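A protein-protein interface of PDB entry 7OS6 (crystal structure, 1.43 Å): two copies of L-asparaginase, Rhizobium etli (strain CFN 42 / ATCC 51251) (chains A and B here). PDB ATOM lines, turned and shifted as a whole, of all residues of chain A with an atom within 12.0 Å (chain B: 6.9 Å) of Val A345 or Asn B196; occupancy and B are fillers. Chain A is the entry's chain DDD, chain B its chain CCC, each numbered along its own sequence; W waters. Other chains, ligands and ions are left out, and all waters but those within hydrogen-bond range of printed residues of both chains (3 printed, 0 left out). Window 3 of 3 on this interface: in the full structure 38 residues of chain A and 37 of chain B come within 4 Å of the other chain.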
ATOM      1  N   ASP A  17      32.956 -29.303   3.811  1.00  0.00           N
ATOM      2  CA  ASP A  17      32.167 -28.070   3.950  1.00  0.00           C
ATOM      3  C   ASP A  17      31.780 -27.568   2.557  1.00  0.00           C
ATOM      4  O   ASP A  17      32.432 -27.912   1.547  1.00  0.00           O
ATOM      5  CB  ASP A  17      32.930 -26.993   4.732  1.00  0.00           C
ATOM      6  CG  ASP A  17      34.073 -26.403   3.919  1.00  0.00           C
ATOM      7  OD1 ASP A  17      35.137 -27.017   3.913  1.00  0.00           O
ATOM      8  OD2 ASP A  17      33.877 -25.333   3.242  1.00  0.00           O
ATOM      9  N   ARG A  18      30.738 -26.748   2.538  1.00  0.00           N
ATOM     10  CA  ARG A  18      30.321 -25.952   1.364  1.00  0.00           C
ATOM     11  C   ARG A  18      30.290 -24.497   1.819  1.00  0.00           C
ATOM     12  O   ARG A  18      29.466 -24.128   2.669  1.00  0.00           O
ATOM     13  CB  ARG A  18      28.964 -26.430   0.861  1.00  0.00           C
ATOM     14  CG  ARG A  18      28.506 -25.813  -0.453  1.00  0.00           C
ATOM     15  CD  ARG A  18      27.256 -26.474  -0.985  1.00  0.00           C
ATOM     16  NE  ARG A  18      27.589 -27.826  -1.377  1.00  0.00           N
ATOM     17  CZ  ARG A  18      28.081 -28.218  -2.571  1.00  0.00           C
ATOM     18  NH1 ARG A  18      28.215 -27.338  -3.556  1.00  0.00           N
ATOM     19  NH2 ARG A  18      28.420 -29.478  -2.764  1.00  0.00           N
ATOM     20  N   GLY A  19      31.245 -23.693   1.347  1.00  0.00           N
ATOM     21  CA  GLY A  19      31.272 -22.279   1.783  1.00  0.00           C
ATOM     22  C   GLY A  19      31.515 -22.149   3.266  1.00  0.00           C
ATOM     23  O   GLY A  19      31.002 -21.165   3.850  1.00  0.00           O
ATOM     24  N   GLY A  20      32.221 -23.104   3.910  1.00  0.00           N
ATOM     25  CA  GLY A  20      32.441 -23.013   5.364  1.00  0.00           C
ATOM     26  C   GLY A  20      31.339 -23.625   6.190  1.00  0.00           C
ATOM     27  O   GLY A  20      31.444 -23.658   7.450  1.00  0.00           O
ATOM     28  N   GLU A  23      29.024 -29.848   5.591  1.00  0.00           N
ATOM     29  CA  GLU A  23      28.236 -30.683   4.652  1.00  0.00           C
ATOM     30  C   GLU A  23      28.089 -32.064   5.310  1.00  0.00           C
ATOM     31  O   GLU A  23      27.029 -32.367   5.880  1.00  0.00           O
ATOM     32  CB  GLU A  23      28.922 -30.715   3.299  1.00  0.00           C
ATOM     33  CG  GLU A  23      28.162 -31.488   2.253  1.00  0.00           C
ATOM     34  CD  GLU A  23      27.330 -30.630   1.321  1.00  0.00           C
ATOM     35  OE1 GLU A  23      27.956 -29.862   0.548  1.00  0.00           O
ATOM     36  OE2 GLU A  23      26.032 -30.592   1.449  1.00  0.00           O
ATOM     37  N   PRO A 337      40.600 -33.714  -2.022  1.00  0.00           N
ATOM     38  CA  PRO A 337      39.806 -33.964  -3.222  1.00  0.00           C
ATOM     39  C   PRO A 337      39.139 -32.670  -3.722  1.00  0.00           C
ATOM     40  O   PRO A 337      38.728 -31.842  -2.898  1.00  0.00           O
ATOM     41  CB  PRO A 337      38.741 -34.961  -2.784  1.00  0.00           C
ATOM     42  CG  PRO A 337      39.137 -35.442  -1.387  1.00  0.00           C
ATOM     43  CD  PRO A 337      40.195 -34.506  -0.842  1.00  0.00           C
ATOM     44  N   GLN A 338      39.045 -32.566  -5.037  1.00  0.00           N
ATOM     45  CA  GLN A 338      38.411 -31.419  -5.743  1.00  0.00           C
ATOM     46  C   GLN A 338      36.977 -31.199  -5.250  1.00  0.00           C
ATOM     47  O   GLN A 338      36.229 -32.171  -5.113  1.00  0.00           O
ATOM     48  CB  GLN A 338      38.399 -31.720  -7.247  1.00  0.00           C
ATOM     49  CG  GLN A 338      39.725 -31.536  -7.949  1.00  0.00           C
ATOM     50  CD  GLN A 338      39.602 -30.407  -8.945  1.00  0.00           C
ATOM     51  OE1 GLN A 338      38.941 -30.522  -9.986  1.00  0.00           O
ATOM     52  NE2 GLN A 338      40.173 -29.272  -8.594  1.00  0.00           N
ATOM     53  N   ARG A 339      36.625 -29.950  -4.969  1.00  0.00           N
ATOM     54  CA  ARG A 339      35.225 -29.541  -4.663  1.00  0.00           C
ATOM     55  C   ARG A 339      34.898 -28.348  -5.562  1.00  0.00           C
ATOM     56  O   ARG A 339      34.817 -27.196  -5.076  1.00  0.00           O
ATOM     57  CB  ARG A 339      35.054 -29.241  -3.171  1.00  0.00           C
ATOM     58  CG  ARG A 339      35.086 -30.477  -2.279  1.00  0.00           C
ATOM     59  CD  ARG A 339      33.902 -31.346  -2.598  1.00  0.00           C
ATOM     60  NE  ARG A 339      33.748 -32.524  -1.764  1.00  0.00           N
ATOM     61  CZ  ARG A 339      34.253 -33.736  -1.980  1.00  0.00           C
ATOM     62  NH1 ARG A 339      35.057 -33.945  -3.011  1.00  0.00           N
ATOM     63  NH2 ARG A 339      33.933 -34.741  -1.180  1.00  0.00           N
ATOM     64  N   VAL A 340      34.796 -28.639  -6.861  1.00  0.00           N
ATOM     65  CA  VAL A 340      34.581 -27.633  -7.934  1.00  0.00           C
ATOM     66  C   VAL A 340      33.242 -27.976  -8.577  1.00  0.00           C
ATOM     67  O   VAL A 340      33.028 -29.174  -8.947  1.00  0.00           O
ATOM     68  CB  VAL A 340      35.745 -27.642  -8.941  1.00  0.00           C
ATOM     69  CG1 VAL A 340      35.516 -26.724 -10.127  1.00  0.00           C
ATOM     70  CG2 VAL A 340      37.072 -27.296  -8.265  1.00  0.00           C
ATOM     71  N   ASN A 341      32.391 -26.968  -8.765  1.00  0.00           N
ATOM     72  CA  ASN A 341      31.030 -27.202  -9.284  1.00  0.00           C
ATOM     73  C   ASN A 341      31.065 -27.345 -10.809  1.00  0.00           C
ATOM     74  O   ASN A 341      32.134 -27.306 -11.430  1.00  0.00           O
ATOM     75  CB  ASN A 341      30.035 -26.172  -8.748  1.00  0.00           C
ATOM     76  CG  ASN A 341      30.169 -24.776  -9.321  1.00  0.00           C
ATOM     77  OD1 ASN A 341      30.905 -24.539 -10.287  1.00  0.00           O
ATOM     78  ND2 ASN A 341      29.413 -23.858  -8.768  1.00  0.00           N
ATOM     79  N   THR A 342      29.885 -27.423 -11.386  1.00  0.00           N
ATOM     80  CA  THR A 342      29.726 -27.693 -12.837  1.00  0.00           C
ATOM     81  C   THR A 342      30.160 -26.475 -13.659  1.00  0.00           C
ATOM     82  O   THR A 342      30.178 -26.613 -14.909  1.00  0.00           O
ATOM     83  CB  THR A 342      28.283 -28.085 -13.151  1.00  0.00           C
ATOM     84  OG1 THR A 342      27.416 -26.994 -12.815  1.00  0.00           O
ATOM     85  CG2 THR A 342      27.830 -29.342 -12.472  1.00  0.00           C
ATOM     86  N   MET A 343      30.435 -25.334 -13.041  1.00  0.00           N
ATOM     87  CA  MET A 343      30.861 -24.098 -13.731  1.00  0.00           C
ATOM     88  C   MET A 343      32.291 -23.736 -13.340  1.00  0.00           C
ATOM     89  O   MET A 343      32.691 -22.604 -13.621  1.00  0.00           O
ATOM     90  CB  MET A 343      29.898 -22.964 -13.424  1.00  0.00           C
ATOM     91  CG  MET A 343      28.489 -23.245 -13.907  1.00  0.00           C
ATOM     92  SD  MET A 343      28.393 -23.316 -15.759  1.00  0.00           S
ATOM     93  CE  MET A 343      28.514 -21.577 -16.090  1.00  0.00           C
ATOM     94  N   GLY A 344      33.023 -24.674 -12.743  1.00  0.00           N
ATOM     95  CA  GLY A 344      34.458 -24.489 -12.449  1.00  0.00           C
ATOM     96  C   GLY A 344      34.709 -23.642 -11.212  1.00  0.00           C
ATOM     97  O   GLY A 344      35.874 -23.233 -10.997  1.00  0.00           O
ATOM     98  N   VAL A 345      33.703 -23.422 -10.363  1.00  0.00           N
ATOM     99  CA  VAL A 345      33.814 -22.600  -9.142  1.00  0.00           C
ATOM    100  C   VAL A 345      34.088 -23.523  -7.951  1.00  0.00           C
ATOM    101  O   VAL A 345      33.379 -24.525  -7.785  1.00  0.00           O
ATOM    102  CB  VAL A 345      32.543 -21.759  -8.927  1.00  0.00           C
ATOM    103  CG1 VAL A 345      32.586 -20.992  -7.616  1.00  0.00           C
ATOM    104  CG2 VAL A 345      32.319 -20.797 -10.090  1.00  0.00           C
ATOM    105  N   THR A 346      35.100 -23.204  -7.146  1.00  0.00           N
ATOM    106  CA  THR A 346      35.418 -24.012  -5.935  1.00  0.00           C
ATOM    107  C   THR A 346      34.378 -23.677  -4.888  1.00  0.00           C
ATOM    108  O   THR A 346      34.179 -22.497  -4.564  1.00  0.00           O
ATOM    109  CB  THR A 346      36.812 -23.747  -5.369  1.00  0.00           C
ATOM    110  OG1 THR A 346      37.745 -24.077  -6.399  1.00  0.00           O
ATOM    111  CG2 THR A 346      37.060 -24.516  -4.092  1.00  0.00           C
ATOM    112  N   THR A 347      33.628 -24.685  -4.431  1.00  0.00           N
ATOM    113  CA  THR A 347      32.475 -24.463  -3.548  1.00  0.00           C
ATOM    114  C   THR A 347      32.733 -24.971  -2.133  1.00  0.00           C
ATOM    115  O   THR A 347      31.931 -24.653  -1.243  1.00  0.00           O
ATOM    116  CB  THR A 347      31.237 -25.166  -4.084  1.00  0.00           C
ATOM    117  OG1 THR A 347      31.547 -26.542  -4.274  1.00  0.00           O
ATOM    118  CG2 THR A 347      30.755 -24.564  -5.374  1.00  0.00           C
ATOM    119  N   GLY A 348      33.785 -25.759  -1.918  1.00  0.00           N
ATOM    120  CA  GLY A 348      33.932 -26.374  -0.604  1.00  0.00           C
ATOM    121  C   GLY A 348      35.276 -27.017  -0.478  1.00  0.00           C
ATOM    122  O   GLY A 348      36.177 -26.688  -1.225  1.00  0.00           O
ATOM    123  N   GLY A 349      35.409 -27.880   0.511  1.00  0.00           N
ATOM    124  CA  GLY A 349      36.683 -28.552   0.738  1.00  0.00           C
ATOM    125  C   GLY A 349      36.582 -29.554   1.867  1.00  0.00           C
ATOM    126  O   GLY A 349      35.499 -29.815   2.355  1.00  0.00           O
ATOM    127  N   ARG B 112      23.385 -20.619 -16.424  1.00  0.00           N
ATOM    128  CA  ARG B 112      24.633 -20.455 -15.635  1.00  0.00           C
ATOM    129  C   ARG B 112      24.852 -21.718 -14.800  1.00  0.00           C
ATOM    130  O   ARG B 112      25.644 -21.623 -13.831  1.00  0.00           O
ATOM    131  CB  ARG B 112      24.550 -19.141 -14.837  1.00  0.00           C
ATOM    132  CG  ARG B 112      24.476 -17.905 -15.736  1.00  0.00           C
ATOM    133  CD  ARG B 112      25.787 -17.585 -16.402  1.00  0.00           C
ATOM    134  NE  ARG B 112      25.638 -16.443 -17.318  1.00  0.00           N
ATOM    135  CZ  ARG B 112      25.408 -16.551 -18.633  1.00  0.00           C
ATOM    136  NH1 ARG B 112      25.308 -17.746 -19.194  1.00  0.00           N
ATOM    137  NH2 ARG B 112      25.276 -15.456 -19.378  1.00  0.00           N
ATOM    138  N   CYS B 113      24.174 -22.821 -15.130  1.00  0.00           N
ATOM    139  CA  CYS B 113      24.471 -24.184 -14.624  1.00  0.00           C
ATOM    140  C   CYS B 113      25.251 -24.961 -15.692  1.00  0.00           C
ATOM    141  O   CYS B 113      25.206 -24.618 -16.906  1.00  0.00           O
ATOM    142  CB  CYS B 113      23.178 -24.927 -14.246  1.00  0.00           C
ATOM    143  SG  CYS B 113      21.941 -25.021 -15.556  1.00  0.00           S
ATOM    144  N   GLY B 114      25.964 -25.991 -15.282  1.00  0.00           N
ATOM    145  CA  GLY B 114      26.742 -26.863 -16.168  1.00  0.00           C
ATOM    146  C   GLY B 114      26.245 -28.289 -16.143  1.00  0.00           C
ATOM    147  O   GLY B 114      25.497 -28.717 -15.254  1.00  0.00           O
ATOM    148  N   HIS B 145      16.842 -23.388 -13.007  1.00  0.00           N
ATOM    149  CA  HIS B 145      17.586 -22.328 -13.735  1.00  0.00           C
ATOM    150  C   HIS B 145      16.696 -21.642 -14.767  1.00  0.00           C
ATOM    151  O   HIS B 145      16.721 -20.396 -14.868  1.00  0.00           O
ATOM    152  CB  HIS B 145      18.866 -22.888 -14.356  1.00  0.00           C
ATOM    153  CG  HIS B 145      19.939 -23.001 -13.317  1.00  0.00           C
ATOM    154  ND1 HIS B 145      20.961 -22.079 -13.245  1.00  0.00           N
ATOM    155  CD2 HIS B 145      20.123 -23.867 -12.283  1.00  0.00           C
ATOM    156  CE1 HIS B 145      21.762 -22.411 -12.232  1.00  0.00           C
ATOM    157  NE2 HIS B 145      21.282 -23.512 -11.650  1.00  0.00           N
ATOM    158  N   HIS B 163      22.061 -15.636 -11.383  1.00  0.00           N
ATOM    159  CA  HIS B 163      22.536 -16.606 -10.359  1.00  0.00           C
ATOM    160  C   HIS B 163      23.331 -15.942  -9.242  1.00  0.00           C
ATOM    161  O   HIS B 163      23.727 -16.646  -8.302  1.00  0.00           O
ATOM    162  CB  HIS B 163      23.344 -17.691 -11.080  1.00  0.00           C
ATOM    163  CG  HIS B 163      24.581 -17.156 -11.674  1.00  0.00           C
ATOM    164  ND1 HIS B 163      24.559 -16.162 -12.648  1.00  0.00           N
ATOM    165  CD2 HIS B 163      25.872 -17.473 -11.454  1.00  0.00           C
ATOM    166  CE1 HIS B 163      25.794 -15.887 -12.988  1.00  0.00           C
ATOM    167  NE2 HIS B 163      26.628 -16.684 -12.270  1.00  0.00           N
ATOM    168  N   LEU B 164      23.633 -14.652  -9.339  1.00  0.00           N
ATOM    169  CA  LEU B 164      24.482 -13.970  -8.337  1.00  0.00           C
ATOM    170  C   LEU B 164      23.646 -13.445  -7.179  1.00  0.00           C
ATOM    171  O   LEU B 164      22.524 -12.958  -7.340  1.00  0.00           O
ATOM    172  CB  LEU B 164      25.256 -12.836  -9.003  1.00  0.00           C
ATOM    173  CG  LEU B 164      26.166 -13.268 -10.158  1.00  0.00           C
ATOM    174  CD1 LEU B 164      26.774 -12.059 -10.829  1.00  0.00           C
ATOM    175  CD2 LEU B 164      27.236 -14.241  -9.681  1.00  0.00           C
ATOM    176  N   THR B 192      27.388 -22.042  -2.229  1.00  0.00           N
ATOM    177  CA  THR B 192      27.144 -22.141  -3.668  1.00  0.00           C
ATOM    178  C   THR B 192      26.950 -23.617  -4.005  1.00  0.00           C
ATOM    179  O   THR B 192      27.765 -24.462  -3.557  1.00  0.00           O
ATOM    180  CB  THR B 192      28.274 -21.495  -4.457  1.00  0.00           C
ATOM    181  OG1 THR B 192      28.360 -20.117  -4.110  1.00  0.00           O
ATOM    182  CG2 THR B 192      28.097 -21.652  -5.952  1.00  0.00           C
ATOM    183  N   ASP B 193      25.935 -23.944  -4.789  1.00  0.00           N
ATOM    184  CA  ASP B 193      25.564 -25.328  -5.134  1.00  0.00           C
ATOM    185  C   ASP B 193      26.364 -25.832  -6.344  1.00  0.00           C
ATOM    186  O   ASP B 193      27.089 -25.067  -7.020  1.00  0.00           O
ATOM    187  CB  ASP B 193      24.064 -25.378  -5.391  1.00  0.00           C
ATOM    188  CG  ASP B 193      23.304 -26.466  -4.703  1.00  0.00           C
ATOM    189  OD1 ASP B 193      23.891 -27.521  -4.577  1.00  0.00           O
ATOM    190  OD2 ASP B 193      22.050 -26.229  -4.453  1.00  0.00           O
ATOM    191  N   GLY B 194      26.194 -27.117  -6.636  1.00  0.00           N
ATOM    192  CA  GLY B 194      26.763 -27.791  -7.811  1.00  0.00           C
ATOM    193  C   GLY B 194      26.336 -27.140  -9.109  1.00  0.00           C
ATOM    194  O   GLY B 194      27.162 -27.046 -10.044  1.00  0.00           O
ATOM    195  N   CYS B 195      25.111 -26.628  -9.122  1.00  0.00           N
ATOM    196  CA  CYS B 195      24.483 -25.952 -10.296  1.00  0.00           C
ATOM    197  C   CYS B 195      24.847 -24.460 -10.363  1.00  0.00           C
ATOM    198  O   CYS B 195      24.332 -23.743 -11.219  1.00  0.00           O
ATOM    199  CB  CYS B 195      22.984 -26.128 -10.246  1.00  0.00           C
ATOM    200  SG  CYS B 195      22.261 -25.213  -8.865  1.00  0.00           S
ATOM    201  N   ASN B 196      25.660 -23.949  -9.434  1.00  0.00           N
ATOM    202  CA  ASN B 196      26.249 -22.585  -9.415  1.00  0.00           C
ATOM    203  C   ASN B 196      25.238 -21.533  -8.940  1.00  0.00           C
ATOM    204  O   ASN B 196      25.505 -20.329  -9.164  1.00  0.00           O
ATOM    205  CB  ASN B 196      26.809 -22.236 -10.776  1.00  0.00           C
ATOM    206  CG  ASN B 196      27.890 -21.192 -10.714  1.00  0.00           C
ATOM    207  OD1 ASN B 196      28.669 -21.113  -9.760  1.00  0.00           O
ATOM    208  ND2 ASN B 196      27.914 -20.352 -11.741  1.00  0.00           N
ATOM    209  N   LEU B 197      24.207 -21.918  -8.210  1.00  0.00           N
ATOM    210  CA  LEU B 197      23.304 -20.946  -7.527  1.00  0.00           C
ATOM    211  C   LEU B 197      23.638 -20.872  -6.045  1.00  0.00           C
ATOM    212  O   LEU B 197      24.109 -21.851  -5.451  1.00  0.00           O
ATOM    213  CB  LEU B 197      21.852 -21.397  -7.650  1.00  0.00           C
ATOM    214  CG  LEU B 197      21.205 -21.154  -9.006  1.00  0.00           C
ATOM    215  CD1 LEU B 197      19.912 -21.928  -9.099  1.00  0.00           C
ATOM    216  CD2 LEU B 197      20.961 -19.658  -9.216  1.00  0.00           C
ATOM    217  N   PRO B 198      23.227 -19.787  -5.374  1.00  0.00           N
ATOM    218  CA  PRO B 198      23.238 -19.719  -3.900  1.00  0.00           C
ATOM    219  C   PRO B 198      22.366 -20.870  -3.376  1.00  0.00           C
ATOM    220  O   PRO B 198      21.335 -21.173  -3.936  1.00  0.00           O
ATOM    221  CB  PRO B 198      22.594 -18.378  -3.578  1.00  0.00           C
ATOM    222  CG  PRO B 198      22.926 -17.572  -4.796  1.00  0.00           C
ATOM    223  CD  PRO B 198      22.693 -18.533  -5.946  1.00  0.00           C
HETATM  224  O   HOH W   1      26.579 -23.217 -18.736  1.00  0.00           O
HETATM  225  O   HOH W   2      24.341 -28.163 -12.831  1.00  0.00           O
HETATM  226  O   HOH W   3      29.981 -22.549  -1.355  1.00  0.00           O
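O of Cys B113 sits close to SD of Met A343, 3.6 Å away. OG1 of Thr A342 sits at hydrogen-bond distance from N of Gly B114, at 3.0 Å. The side-chain sulfur of Met A343 lies within hydrogen-bond range of the backbone NH of Gly B114 (3.6 Å). The guanidinium group of Arg A18 is in hydrogen-bond range of the backbone carbonyl oxygen of Thr B192 (2.9 Å). The backbone carbonyl oxygen (O) of Arg B112 lies close to the side-chain sulfur (SD) of Met A343 (3.8 Å). ND2 of Asn A341 lies within hydrogen-bond range of O of Asp B193, at 3.1 Å. ND2 of Asn A341 sits at hydrogen-bond distance from OD1 of Asn B196. The side-chain hydroxyl (OG1) of Thr A342 sits at hydrogen-bond distance from the backbone carbonyl oxygen (O) of Gly B194 (2.8 Å).
The guanidinium group (NH1) of Arg A18 sits close to the side-chain hydroxyl (OG1) of Thr A347. The side-chain amide oxygen of Asn A341 lies within hydrogen-bond range of the backbone NH of Met A343 (2.9 Å). The backbone carbonyl oxygen of Arg B112 lies close to the side-chain amide nitrogen of Asn B196, at 3.3 Å. The side-chain amide oxygen (OD1) of Asn A341 lies within hydrogen-bond range of the backbone NH (N) of Gly A344, at 3.2 Å. The backbone carbonyl oxygen (O) of Arg A339 is in hydrogen-bond range of the backbone NH (N) of Thr A347 (2.9 Å). The backbone carbonyl oxygen (O) of Thr A347 lies within hydrogen-bond range of the backbone NH (N) of Gly A19, 2.8 Å away.
Printed residues of chain B within 4 Å of Arg A18: Thr B192, Asp B193 and Gly B194. Pro A337 touches none of the printed residues of chain B. No residue of chain B comes within 4 Å of Gly A344. Printed residues of chain B within 4 Å of Val A345: Asn B196. Of the printed residues of chain A, Arg B112 touches Met A343. Of chain A, only Met A343 comes within 4 Å of Cys B113. His B145 touches none of the printed residues of chain A. Thr B192 touches just these residues of chain A: Arg A18 (2.9 Å), Asn A341 (3.8 Å) and Thr A347 (3.5 Å). Gly B194 touches just these residues of chain A: Arg A18 (3.7 Å), Asn A341 (3.3 Å) and Thr A342 (2.8 Å). Asn B196 touches three residues of chain A. No residue of chain A comes within 4 Å of Leu B197. No residue of chain A comes within 4 Å of Pro B198. The nearest residue of chain B that does not touch Val A345 is Thr B192 (4.8 Å). The nearest residue of chain A that does not touch Asn B196 is Thr A342 (4.9 Å).
Among the printed residues, pairs that only touch across the chains: Asn A341 with Gly B194 (3.3 Å), Thr A347 with Thr B192 (3.5 Å), Met A343 with Asn B196 (3.7 Å), Arg A18 with Asp B193 (3.7 Å), Val A345 with Asn B196 (3.7 Å), Arg A18 with Gly B194 (3.7 Å) and Asn A341 with Thr B192 (3.8 Å).
Hydrophobic or aromatic side chains of chain A within 4 Å of the printed part of chain B: Met A343 and Val A345. Of the 13 printed residues of chain B, 7 touch a printed residue of chain A. Among the printed residues, 15 pairs touch across the chains. Among the printed residues, no Asp or Glu carboxylate lies within 4 Å of a Lys or Arg side-chain nitrogen of the other chain.
No position is printed for both chains. Of the 15 pairs that touch across the chains among the printed residues, none has its exchanged pair printed and touching as well.
Water W1 bridges O of Cys B113 (2.7 Å) and SD of Met A343 (3.5 Å). Water W2 lies within hydrogen-bond range of the backbone carbonyl oxygen of Gly B114 (2.7 Å) and the side-chain hydroxyl of Thr A342 (3.3 Å). Water W3 lies within hydrogen-bond range of N of Thr B192 (2.8 Å), O of Thr A347 (2.9 Å) and N of Gly A19 (3.2 Å).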
